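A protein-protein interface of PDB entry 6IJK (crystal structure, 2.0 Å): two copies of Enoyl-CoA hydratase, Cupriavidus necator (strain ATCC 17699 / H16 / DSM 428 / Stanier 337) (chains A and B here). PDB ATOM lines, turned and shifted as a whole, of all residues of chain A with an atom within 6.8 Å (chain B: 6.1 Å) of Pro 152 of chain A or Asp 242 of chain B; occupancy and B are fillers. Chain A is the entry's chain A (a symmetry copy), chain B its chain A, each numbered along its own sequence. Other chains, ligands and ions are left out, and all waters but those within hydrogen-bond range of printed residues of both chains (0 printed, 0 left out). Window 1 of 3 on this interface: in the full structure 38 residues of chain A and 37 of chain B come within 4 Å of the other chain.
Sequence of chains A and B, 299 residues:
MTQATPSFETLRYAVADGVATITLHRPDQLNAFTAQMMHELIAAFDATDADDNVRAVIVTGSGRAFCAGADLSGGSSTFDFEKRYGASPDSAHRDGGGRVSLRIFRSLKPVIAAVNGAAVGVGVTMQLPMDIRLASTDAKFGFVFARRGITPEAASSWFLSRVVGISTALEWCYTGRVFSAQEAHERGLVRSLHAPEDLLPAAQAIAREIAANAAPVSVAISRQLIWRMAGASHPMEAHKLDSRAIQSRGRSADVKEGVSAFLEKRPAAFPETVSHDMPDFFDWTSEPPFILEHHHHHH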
ATOM      1  N   ASP A  95      30.246  -8.025 -33.587  1.00  0.00           N
ATOM      2  CA  ASP A  95      29.439  -9.057 -32.905  1.00  0.00           C
ATOM      3  C   ASP A  95      29.121 -10.094 -33.967  1.00  0.00           C
ATOM      4  O   ASP A  95      28.745  -9.708 -35.088  1.00  0.00           O
ATOM      5  CB  ASP A  95      28.235  -8.384 -32.234  1.00  0.00           C
ATOM      6  CG  ASP A  95      27.218  -9.367 -31.704  1.00  0.00           C
ATOM      7  OD1 ASP A  95      27.572 -10.100 -30.817  1.00  0.00           O
ATOM      8  OD2 ASP A  95      26.099  -9.403 -32.239  1.00  0.00           O
ATOM      9  N   GLY A  98      25.348 -10.007 -35.176  1.00  0.00           N
ATOM     10  CA  GLY A  98      25.158  -8.861 -36.075  1.00  0.00           C
ATOM     11  C   GLY A  98      25.561  -9.160 -37.471  1.00  0.00           C
ATOM     12  O   GLY A  98      24.872  -8.655 -38.399  1.00  0.00           O
ATOM     13  N   THR A 125      17.436 -13.314 -31.236  1.00  0.00           N
ATOM     14  CA  THR A 125      17.845 -12.038 -31.896  1.00  0.00           C
ATOM     15  C   THR A 125      18.086 -12.303 -33.383  1.00  0.00           C
ATOM     16  O   THR A 125      17.737 -11.421 -34.196  1.00  0.00           O
ATOM     17  CB  THR A 125      18.938 -11.292 -31.127  1.00  0.00           C
ATOM     18  OG1 THR A 125      20.069 -12.127 -31.060  1.00  0.00           O
ATOM     19  CG2 THR A 125      18.548 -10.896 -29.721  1.00  0.00           C
ATOM     20  N   PHE A 143      15.056 -13.036 -24.181  1.00  0.00           N
ATOM     21  CA  PHE A 143      16.163 -12.081 -24.397  1.00  0.00           C
ATOM     22  C   PHE A 143      16.889 -11.999 -23.062  1.00  0.00           C
ATOM     23  O   PHE A 143      16.588 -11.092 -22.308  1.00  0.00           O
ATOM     24  CB  PHE A 143      15.613 -10.730 -24.853  1.00  0.00           C
ATOM     25  CG  PHE A 143      14.840 -10.783 -26.146  1.00  0.00           C
ATOM     26  CD1 PHE A 143      13.551 -11.301 -26.187  1.00  0.00           C
ATOM     27  CD2 PHE A 143      15.401 -10.300 -27.322  1.00  0.00           C
ATOM     28  CE1 PHE A 143      12.839 -11.312 -27.375  1.00  0.00           C
ATOM     29  CE2 PHE A 143      14.710 -10.373 -28.525  1.00  0.00           C
ATOM     30  CZ  PHE A 143      13.425 -10.859 -28.537  1.00  0.00           C
ATOM     31  N   PHE A 145      19.973 -11.753 -22.024  1.00  0.00           N
ATOM     32  CA  PHE A 145      21.251 -11.000 -21.897  1.00  0.00           C
ATOM     33  C   PHE A 145      21.419 -10.370 -20.512  1.00  0.00           C
ATOM     34  O   PHE A 145      22.442 -10.690 -19.859  1.00  0.00           O
ATOM     35  CB  PHE A 145      21.360  -9.939 -22.976  1.00  0.00           C
ATOM     36  CG  PHE A 145      21.061 -10.514 -24.324  1.00  0.00           C
ATOM     37  CD1 PHE A 145      22.040 -11.195 -25.021  1.00  0.00           C
ATOM     38  CD2 PHE A 145      19.774 -10.493 -24.821  1.00  0.00           C
ATOM     39  CE1 PHE A 145      21.756 -11.737 -26.261  1.00  0.00           C
ATOM     40  CE2 PHE A 145      19.512 -10.996 -26.079  1.00  0.00           C
ATOM     41  CZ  PHE A 145      20.502 -11.618 -26.794  1.00  0.00           C
ATOM     42  N   ALA A 146      20.516  -9.482 -20.082  1.00  0.00           N
ATOM     43  CA  ALA A 146      20.743  -8.698 -18.847  1.00  0.00           C
ATOM     44  C   ALA A 146      20.876  -9.638 -17.618  1.00  0.00           C
ATOM     45  O   ALA A 146      21.674  -9.333 -16.738  1.00  0.00           O
ATOM     46  CB  ALA A 146      19.694  -7.631 -18.705  1.00  0.00           C
ATOM     47  N   ILE A 150      25.278  -9.344 -19.738  1.00  0.00           N
ATOM     48  CA  ILE A 150      25.643  -8.860 -21.105  1.00  0.00           C
ATOM     49  C   ILE A 150      24.452  -8.098 -21.689  1.00  0.00           C
ATOM     50  O   ILE A 150      23.538  -7.751 -20.911  1.00  0.00           O
ATOM     51  CB  ILE A 150      26.174 -10.007 -21.983  1.00  0.00           C
ATOM     52  CG1 ILE A 150      25.180 -11.140 -22.215  1.00  0.00           C
ATOM     53  CG2 ILE A 150      27.448 -10.575 -21.399  1.00  0.00           C
ATOM     54  CD1 ILE A 150      25.602 -12.048 -23.380  1.00  0.00           C
ATOM     55  N   THR A 151      24.472  -7.856 -22.999  1.00  0.00           N
ATOM     56  CA  THR A 151      23.568  -6.917 -23.707  1.00  0.00           C
ATOM     57  C   THR A 151      23.012  -7.552 -24.982  1.00  0.00           C
ATOM     58  O   THR A 151      23.678  -8.347 -25.636  1.00  0.00           O
ATOM     59  CB  THR A 151      24.282  -5.573 -23.951  1.00  0.00           C
ATOM     60  OG1 THR A 151      25.595  -5.735 -24.499  1.00  0.00           O
ATOM     61  CG2 THR A 151      24.438  -4.791 -22.674  1.00  0.00           C
ATOM     62  N   PRO A 152      21.770  -7.193 -25.374  1.00  0.00           N
ATOM     63  CA  PRO A 152      21.181  -7.660 -26.615  1.00  0.00           C
ATOM     64  C   PRO A 152      22.090  -7.264 -27.774  1.00  0.00           C
ATOM     65  O   PRO A 152      22.562  -6.131 -27.823  1.00  0.00           O
ATOM     66  CB  PRO A 152      19.814  -6.952 -26.714  1.00  0.00           C
ATOM     67  CG  PRO A 152      19.520  -6.497 -25.322  1.00  0.00           C
ATOM     68  CD  PRO A 152      20.869  -6.255 -24.672  1.00  0.00           C
ATOM     69  N   GLU A 153      22.313  -8.229 -28.659  1.00  0.00           N
ATOM     70  CA  GLU A 153      23.236  -8.109 -29.818  1.00  0.00           C
ATOM     71  C   GLU A 153      22.467  -8.433 -31.111  1.00  0.00           C
ATOM     72  O   GLU A 153      21.223  -8.401 -31.113  1.00  0.00           O
ATOM     73  CB  GLU A 153      24.478  -8.983 -29.556  1.00  0.00           C
ATOM     74  CG  GLU A 153      24.173 -10.324 -28.896  1.00  0.00           C
ATOM     75  CD  GLU A 153      23.168 -11.178 -29.658  1.00  0.00           C
ATOM     76  OE1 GLU A 153      23.606 -12.221 -30.208  1.00  0.00           O
ATOM     77  OE2 GLU A 153      21.945 -10.783 -29.726  1.00  0.00           O
ATOM     78  N   ALA A 154      23.203  -8.690 -32.183  1.00  0.00           N
ATOM     79  CA  ALA A 154      22.707  -9.033 -33.530  1.00  0.00           C
ATOM     80  C   ALA A 154      21.877  -7.869 -34.062  1.00  0.00           C
ATOM     81  O   ALA A 154      20.930  -8.134 -34.816  1.00  0.00           O
ATOM     82  CB  ALA A 154      21.898 -10.329 -33.502  1.00  0.00           C
ATOM     83  N   ALA A 155      22.218  -6.639 -33.644  1.00  0.00           N
ATOM     84  CA  ALA A 155      21.536  -5.385 -34.028  1.00  0.00           C
ATOM     85  C   ALA A 155      20.073  -5.435 -33.564  1.00  0.00           C
ATOM     86  O   ALA A 155      19.271  -4.681 -34.135  1.00  0.00           O
ATOM     87  CB  ALA A 155      21.653  -5.181 -35.501  1.00  0.00           C
ATOM     88  N   SER A 156      19.750  -6.224 -32.522  1.00  0.00           N
ATOM     89  CA  SER A 156      18.358  -6.377 -32.003  1.00  0.00           C
ATOM     90  C   SER A 156      17.828  -5.029 -31.466  1.00  0.00           C
ATOM     91  O   SER A 156      16.608  -4.809 -31.457  1.00  0.00           O
ATOM     92  CB  SER A 156      18.317  -7.475 -30.952  1.00  0.00           C
ATOM     93  OG  SER A 156      19.051  -7.082 -29.805  1.00  0.00           O
ATOM     94  N   SER A 157      18.704  -4.142 -30.984  1.00  0.00           N
ATOM     95  CA  SER A 157      18.301  -2.780 -30.606  1.00  0.00           C
ATOM     96  C   SER A 157      17.654  -2.070 -31.811  1.00  0.00           C
ATOM     97  O   SER A 157      16.861  -1.178 -31.552  1.00  0.00           O
ATOM     98  CB  SER A 157      19.453  -2.000 -30.025  1.00  0.00           C
ATOM     99  OG  SER A 157      20.433  -1.795 -31.003  1.00  0.00           O
ATOM    100  N   TRP A 158      17.964  -2.425 -33.075  1.00  0.00           N
ATOM    101  CA  TRP A 158      17.263  -1.873 -34.267  1.00  0.00           C
ATOM    102  C   TRP A 158      16.026  -2.713 -34.632  1.00  0.00           C
ATOM    103  O   TRP A 158      14.989  -2.116 -34.867  1.00  0.00           O
ATOM    104  CB  TRP A 158      18.184  -1.732 -35.472  1.00  0.00           C
ATOM    105  CG  TRP A 158      17.615  -0.921 -36.587  1.00  0.00           C
ATOM    106  CD1 TRP A 158      17.725   0.426 -36.741  1.00  0.00           C
ATOM    107  CD2 TRP A 158      16.872  -1.383 -37.725  1.00  0.00           C
ATOM    108  NE1 TRP A 158      17.188   0.829 -37.927  1.00  0.00           N
ATOM    109  CE2 TRP A 158      16.590  -0.253 -38.517  1.00  0.00           C
ATOM    110  CE3 TRP A 158      16.447  -2.636 -38.176  1.00  0.00           C
ATOM    111  CZ2 TRP A 158      15.906  -0.344 -39.724  1.00  0.00           C
ATOM    112  CZ3 TRP A 158      15.757  -2.714 -39.361  1.00  0.00           C
ATOM    113  CH2 TRP A 158      15.503  -1.591 -40.128  1.00  0.00           C
ATOM    114  N   LEU A 160      14.246  -5.251 -33.003  1.00  0.00           N
ATOM    115  CA  LEU A 160      13.236  -5.801 -32.048  1.00  0.00           C
ATOM    116  C   LEU A 160      12.073  -4.806 -31.923  1.00  0.00           C
ATOM    117  O   LEU A 160      10.940  -5.254 -32.057  1.00  0.00           O
ATOM    118  CB  LEU A 160      13.825  -6.172 -30.677  1.00  0.00           C
ATOM    119  CG  LEU A 160      12.799  -6.834 -29.738  1.00  0.00           C
ATOM    120  CD1 LEU A 160      12.355  -8.213 -30.236  1.00  0.00           C
ATOM    121  CD2 LEU A 160      13.328  -6.941 -28.329  1.00  0.00           C
ATOM    122  N   CYS A 173      13.741  -7.338 -22.569  1.00  0.00           N
ATOM    123  CA  CYS A 173      15.222  -7.186 -22.383  1.00  0.00           C
ATOM    124  C   CYS A 173      15.551  -6.803 -20.930  1.00  0.00           C
ATOM    125  O   CYS A 173      16.607  -7.210 -20.463  1.00  0.00           O
ATOM    126  CB  CYS A 173      15.823  -6.178 -23.355  1.00  0.00           C
ATOM    127  SG  CYS A 173      15.736  -6.686 -25.092  1.00  0.00           S
ATOM    128  N   SER B 218      23.845  -3.487 -17.827  1.00  0.00           N
ATOM    129  CA  SER B 218      23.219  -4.137 -19.018  1.00  0.00           C
ATOM    130  C   SER B 218      21.839  -3.538 -19.297  1.00  0.00           C
ATOM    131  O   SER B 218      21.546  -3.203 -20.457  1.00  0.00           O
ATOM    132  CB  SER B 218      23.113  -5.632 -18.874  1.00  0.00           C
ATOM    133  OG  SER B 218      24.379  -6.211 -18.974  1.00  0.00           O
ATOM    134  N   SER B 222      20.906  -1.375 -22.663  1.00  0.00           N
ATOM    135  CA  SER B 222      19.715  -1.869 -23.407  1.00  0.00           C
ATOM    136  C   SER B 222      18.717  -0.728 -23.602  1.00  0.00           C
ATOM    137  O   SER B 222      18.221  -0.538 -24.742  1.00  0.00           O
ATOM    138  CB  SER B 222      19.020  -3.019 -22.694  1.00  0.00           C
ATOM    139  OG  SER B 222      19.826  -4.171 -22.652  1.00  0.00           O
ATOM    140  N   LEU B 225      20.116   1.843 -26.147  1.00  0.00           N
ATOM    141  CA  LEU B 225      20.187   1.394 -27.556  1.00  0.00           C
ATOM    142  C   LEU B 225      18.778   1.198 -28.103  1.00  0.00           C
ATOM    143  O   LEU B 225      18.537   1.567 -29.254  1.00  0.00           O
ATOM    144  CB  LEU B 225      21.048   0.126 -27.638  1.00  0.00           C
ATOM    145  CG  LEU B 225      22.521   0.345 -27.281  1.00  0.00           C
ATOM    146  CD1 LEU B 225      23.334  -0.917 -27.502  1.00  0.00           C
ATOM    147  CD2 LEU B 225      23.120   1.492 -28.081  1.00  0.00           C
ATOM    148  N   ILE B 226      17.835   0.665 -27.319  1.00  0.00           N
ATOM    149  CA  ILE B 226      16.498   0.398 -27.918  1.00  0.00           C
ATOM    150  C   ILE B 226      15.837   1.736 -28.293  1.00  0.00           C
ATOM    151  O   ILE B 226      15.303   1.867 -29.427  1.00  0.00           O
ATOM    152  CB  ILE B 226      15.644  -0.490 -26.999  1.00  0.00           C
ATOM    153  CG1 ILE B 226      16.193  -1.924 -27.002  1.00  0.00           C
ATOM    154  CG2 ILE B 226      14.196  -0.399 -27.451  1.00  0.00           C
ATOM    155  CD1 ILE B 226      15.621  -2.841 -25.900  1.00  0.00           C
ATOM    156  N   GLU B 237      23.931   0.860 -37.702  1.00  0.00           N
ATOM    157  CA  GLU B 237      24.159   1.784 -36.572  1.00  0.00           C
ATOM    158  C   GLU B 237      24.109   1.002 -35.263  1.00  0.00           C
ATOM    159  O   GLU B 237      24.979   1.240 -34.409  1.00  0.00           O
ATOM    160  CB  GLU B 237      23.153   2.932 -36.548  1.00  0.00           C
ATOM    161  CG  GLU B 237      23.458   3.998 -37.576  1.00  0.00           C
ATOM    162  CD  GLU B 237      24.839   4.594 -37.387  1.00  0.00           C
ATOM    163  OE1 GLU B 237      25.349   4.558 -36.230  1.00  0.00           O
ATOM    164  OE2 GLU B 237      25.422   5.058 -38.388  1.00  0.00           O
ATOM    165  N   ALA B 238      23.119   0.113 -35.112  1.00  0.00           N
ATOM    166  CA  ALA B 238      22.951  -0.697 -33.898  1.00  0.00           C
ATOM    167  C   ALA B 238      24.121  -1.674 -33.812  1.00  0.00           C
ATOM    168  O   ALA B 238      24.658  -1.903 -32.723  1.00  0.00           O
ATOM    169  CB  ALA B 238      21.626  -1.416 -33.947  1.00  0.00           C
ATOM    170  N   HIS B 239      24.499  -2.266 -34.932  1.00  0.00           N
ATOM    171  CA  HIS B 239      25.572  -3.292 -34.941  1.00  0.00           C
ATOM    172  C   HIS B 239      26.879  -2.676 -34.409  1.00  0.00           C
ATOM    173  O   HIS B 239      27.563  -3.342 -33.646  1.00  0.00           O
ATOM    174  CB  HIS B 239      25.688  -3.912 -36.323  1.00  0.00           C
ATOM    175  CG  HIS B 239      26.813  -4.881 -36.504  1.00  0.00           C
ATOM    176  ND1 HIS B 239      26.975  -5.996 -35.707  1.00  0.00           N
ATOM    177  CD2 HIS B 239      27.789  -4.936 -37.437  1.00  0.00           C
ATOM    178  CE1 HIS B 239      28.028  -6.679 -36.123  1.00  0.00           C
ATOM    179  NE2 HIS B 239      28.533  -6.056 -37.189  1.00  0.00           N
ATOM    180  N   LYS B 240      27.194  -1.444 -34.790  1.00  0.00           N
ATOM    181  CA  LYS B 240      28.433  -0.742 -34.388  1.00  0.00           C
ATOM    182  C   LYS B 240      28.392  -0.558 -32.882  1.00  0.00           C
ATOM    183  O   LYS B 240      29.365  -0.961 -32.239  1.00  0.00           O
ATOM    184  CB  LYS B 240      28.573   0.610 -35.098  1.00  0.00           C
ATOM    185  CG  LYS B 240      28.834   0.496 -36.590  1.00  0.00           C
ATOM    186  CD  LYS B 240      29.025   1.813 -37.269  1.00  0.00           C
ATOM    187  CE  LYS B 240      27.727   2.579 -37.408  1.00  0.00           C
ATOM    188  NZ  LYS B 240      27.986   3.975 -37.840  1.00  0.00           N
ATOM    189  N   LEU B 241      27.313   0.018 -32.344  1.00  0.00           N
ATOM    190  CA  LEU B 241      27.187   0.282 -30.894  1.00  0.00           C
ATOM    191  C   LEU B 241      27.111  -1.047 -30.140  1.00  0.00           C
ATOM    192  O   LEU B 241      27.759  -1.179 -29.109  1.00  0.00           O
ATOM    193  CB  LEU B 241      25.951   1.146 -30.581  1.00  0.00           C
ATOM    194  CG  LEU B 241      25.968   2.560 -31.161  1.00  0.00           C
ATOM    195  CD1 LEU B 241      24.595   3.180 -31.150  1.00  0.00           C
ATOM    196  CD2 LEU B 241      26.965   3.459 -30.433  1.00  0.00           C
ATOM    197  N   ASP B 242      26.282  -1.993 -30.582  1.00  0.00           N
ATOM    198  CA  ASP B 242      26.032  -3.206 -29.755  1.00  0.00           C
ATOM    199  C   ASP B 242      27.264  -4.130 -29.852  1.00  0.00           C
ATOM    200  O   ASP B 242      27.445  -4.963 -28.936  1.00  0.00           O
ATOM    201  CB  ASP B 242      24.653  -3.815 -30.077  1.00  0.00           C
ATOM    202  CG  ASP B 242      24.673  -4.741 -31.282  1.00  0.00           C
ATOM    203  OD1 ASP B 242      25.790  -5.001 -31.787  1.00  0.00           O
ATOM    204  OD2 ASP B 242      23.584  -5.220 -31.694  1.00  0.00           O
ATOM    205  N   SER B 243      28.114  -3.992 -30.879  1.00  0.00           N
ATOM    206  CA  SER B 243      29.428  -4.684 -30.921  1.00  0.00           C
ATOM    207  C   SER B 243      30.321  -4.155 -29.787  1.00  0.00           C
ATOM    208  O   SER B 243      30.912  -4.979 -29.065  1.00  0.00           O
ATOM    209  CB  SER B 243      30.062  -4.542 -32.264  1.00  0.00           C
ATOM    210  OG  SER B 243      29.303  -5.272 -33.225  1.00  0.00           O
ATOM    211  N   ARG B 244      30.388  -2.833 -29.588  1.00  0.00           N
ATOM    212  CA  ARG B 244      31.230  -2.218 -28.537  1.00  0.00           C
ATOM    213  C   ARG B 244      30.616  -2.595 -27.172  1.00  0.00           C
ATOM    214  O   ARG B 244      31.372  -2.898 -26.221  1.00  0.00           O
ATOM    215  CB  ARG B 244      31.337  -0.698 -28.735  1.00  0.00           C
ATOM    216  CG  ARG B 244      32.050  -0.219 -30.001  1.00  0.00           C
ATOM    217  CD  ARG B 244      33.558  -0.464 -30.046  1.00  0.00           C
ATOM    218  NE  ARG B 244      34.282  -0.033 -28.851  1.00  0.00           N
ATOM    219  CZ  ARG B 244      34.730   1.205 -28.596  1.00  0.00           C
ATOM    220  NH1 ARG B 244      34.543   2.197 -29.448  1.00  0.00           N
ATOM    221  NH2 ARG B 244      35.371   1.449 -27.464  1.00  0.00           N
ATOM    222  N   ALA B 245      29.286  -2.579 -27.036  1.00  0.00           N
ATOM    223  CA  ALA B 245      28.618  -2.860 -25.742  1.00  0.00           C
ATOM    224  C   ALA B 245      28.949  -4.292 -25.284  1.00  0.00           C
ATOM    225  O   ALA B 245      29.249  -4.443 -24.108  1.00  0.00           O
ATOM    226  CB  ALA B 245      27.123  -2.638 -25.803  1.00  0.00           C
ATOM    227  N   ILE B 246      28.840  -5.286 -26.173  1.00  0.00           N
ATOM    228  CA  ILE B 246      28.988  -6.742 -25.843  1.00  0.00           C
ATOM    229  C   ILE B 246      30.476  -7.072 -25.589  1.00  0.00           C
ATOM    230  O   ILE B 246      30.734  -7.905 -24.714  1.00  0.00           O
ATOM    231  CB  ILE B 246      28.366  -7.647 -26.927  1.00  0.00           C
ATOM    232  CG1 ILE B 246      28.186  -9.089 -26.439  1.00  0.00           C
ATOM    233  CG2 ILE B 246      29.180  -7.606 -28.207  1.00  0.00           C
ATOM    234  CD1 ILE B 246      26.861  -9.343 -25.780  1.00  0.00           C
ATOM    235  N   GLN B 247      31.402  -6.441 -26.324  1.00  0.00           N
ATOM    236  CA  GLN B 247      32.870  -6.485 -26.084  1.00  0.00           C
ATOM    237  C   GLN B 247      33.175  -6.017 -24.650  1.00  0.00           C
ATOM    238  O   GLN B 247      33.881  -6.739 -23.912  1.00  0.00           O
ATOM    239  CB  GLN B 247      33.564  -5.609 -27.128  1.00  0.00           C
ATOM    240  CG  GLN B 247      35.083  -5.611 -27.049  1.00  0.00           C
ATOM    241  CD  GLN B 247      35.673  -4.591 -27.993  1.00  0.00           C
ATOM    242  OE1 GLN B 247      36.413  -4.933 -28.918  1.00  0.00           O
ATOM    243  NE2 GLN B 247      35.339  -3.324 -27.772  1.00  0.00           N
ATOM    244  N   PHE B 281      32.746   4.348 -24.354  1.00  0.00           N
ATOM    245  CA  PHE B 281      32.815   4.471 -25.839  1.00  0.00           C
ATOM    246  C   PHE B 281      31.637   5.293 -26.389  1.00  0.00           C
ATOM    247  O   PHE B 281      31.649   5.604 -27.588  1.00  0.00           O
ATOM    248  CB  PHE B 281      32.852   3.096 -26.517  1.00  0.00           C
ATOM    249  CG  PHE B 281      31.575   2.310 -26.382  1.00  0.00           C
ATOM    250  CD1 PHE B 281      30.508   2.537 -27.234  1.00  0.00           C
ATOM    251  CD2 PHE B 281      31.430   1.369 -25.377  1.00  0.00           C
ATOM    252  CE1 PHE B 281      29.323   1.848 -27.080  1.00  0.00           C
ATOM    253  CE2 PHE B 281      30.252   0.649 -25.245  1.00  0.00           C
ATOM    254  CZ  PHE B 281      29.202   0.886 -26.104  1.00  0.00           C
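The side-chain hydroxyl of Ser 222 of chain B lies within hydrogen-bond range of the backbone carbonyl oxygen of Ser 218 of chain B.
O of His 239 of chain B sits at hydrogen-bond distance from OG of Ser 243 of chain B, at 2.6 Å.
OD2 of Asp 95 of chain A is in hydrogen-bond range of N of Gly 98 of chain A (3.1 Å).
The side-chain carboxylate (OE2) of Glu 153 of chain A lies within hydrogen-bond range of the side-chain hydroxyl (OG1) of Thr 125 of chain A, at 2.7 Å.
O of Phe 145 of chain A sits at hydrogen-bond distance from N of Ile 150 of chain A (3.1 Å).
The backbone carbonyl oxygen (O) of Glu 153 of chain A sits at hydrogen-bond distance from the side-chain hydroxyl (OG) of Ser 156 of chain A (2.9 Å).
The side-chain hydroxyl (OG) of Ser 218 of chain B lies within hydrogen-bond range of the backbone carbonyl oxygen (O) of Ile 150 of chain A (2.6 Å).
N of Ala 155 of chain A is in hydrogen-bond range of OD2 of Asp 242 of chain B.
The backbone NH of Asp 95 of chain A sits at hydrogen-bond distance from the side-chain hydroxyl of Ser 243 of chain B (2.9 Å).
O of Asp 95 of chain A touches CE1 of His 239 of chain B (3.3 Å).
Gly 98 of chain A touches His 239 of chain B.
CA of Ala 146 of chain A touches CB of Ser 218 of chain B (3.9 Å).
Ile 150 of chain A touches Ile 246 of chain B (CD1 to CD1, 3.8 Å).
Pro 152 of chain A touches Asp 242 of chain B.
C of Glu 153 of chain A touches OD2 of Asp 242 of chain B (3.5 Å).
Ala 154 of chain A touches Asp 242 of chain B (N to OD2, 3.5 Å).
O of Ser 157 of chain A touches CA of Ile 226 of chain B, at 3.98 Å.
Ala 238 of chain B touches Ser 157 of chain A.
Ala 238 of chain B touches Trp 158 of chain A.
Of the 17 printed residues of chain A, 12 touch a printed residue of chain B.
Printed residues of chain A that touch a printed residue of chain B: Asp 95, Gly 98, Ala 146, Ile 150, Thr 151, Pro 152, Glu 153, Ala 154, Ala 155, Ser 157, Trp 158 and Cys 173.
Hydrophobic or aromatic side chains of chain A within 4 Å of the printed part of chain B: Ala 146, Ile 150, Pro 152 and Trp 158.
Printed residues of chain B that touch a printed residue of chain A: Ser 218, Ser 222, Leu 225, Ile 226, Ala 238, His 239, Asp 242, Ser 243, Ala 245 and Ile 246.
Hydrophobic or aromatic side chains of chain B that line the printed part of chain A: Leu 225, Ile 226, Ala 238, His 239, Ala 245 and Ile 246.
No position is printed for both chains.
Of the 21 pairs that touch across the chains among the printed residues, none has its exchanged pair printed and touching as well.
Pro 152 of chain A touches just these residues of chain B: Ser 222 and Asp 242.
Of chain A, only Pro 152 (3.8 Å), Glu 153 (3.5 Å), Ala 154 (3.5 Å) and Ala 155 (2.8 Å) come within 4 Å of Asp 242 of chain B.
Printed residues of chain B within 4 Å of Ile 150 of chain A: Ser 218 (2.6 Å) and Ile 246 (3.8 Å).
Of the printed residues of chain B, Thr 151 of chain A touches Ser 218 (3.9 Å), Ala 245 (3.7 Å) and Ile 246 (3.3 Å).
Printed residues of chain A within 4 Å of Ser 222 of chain B: Pro 152.
Printed residues of chain B within 4 Å of Ala 155 of chain A: Ala 238 and Asp 242.
Printed residues of chain B within 4 Å of Gly 98 of chain A: His 239.
The nearest residue of chain B that does not touch Pro 152 of chain A is Ser 218 of chain B (5.2 Å).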
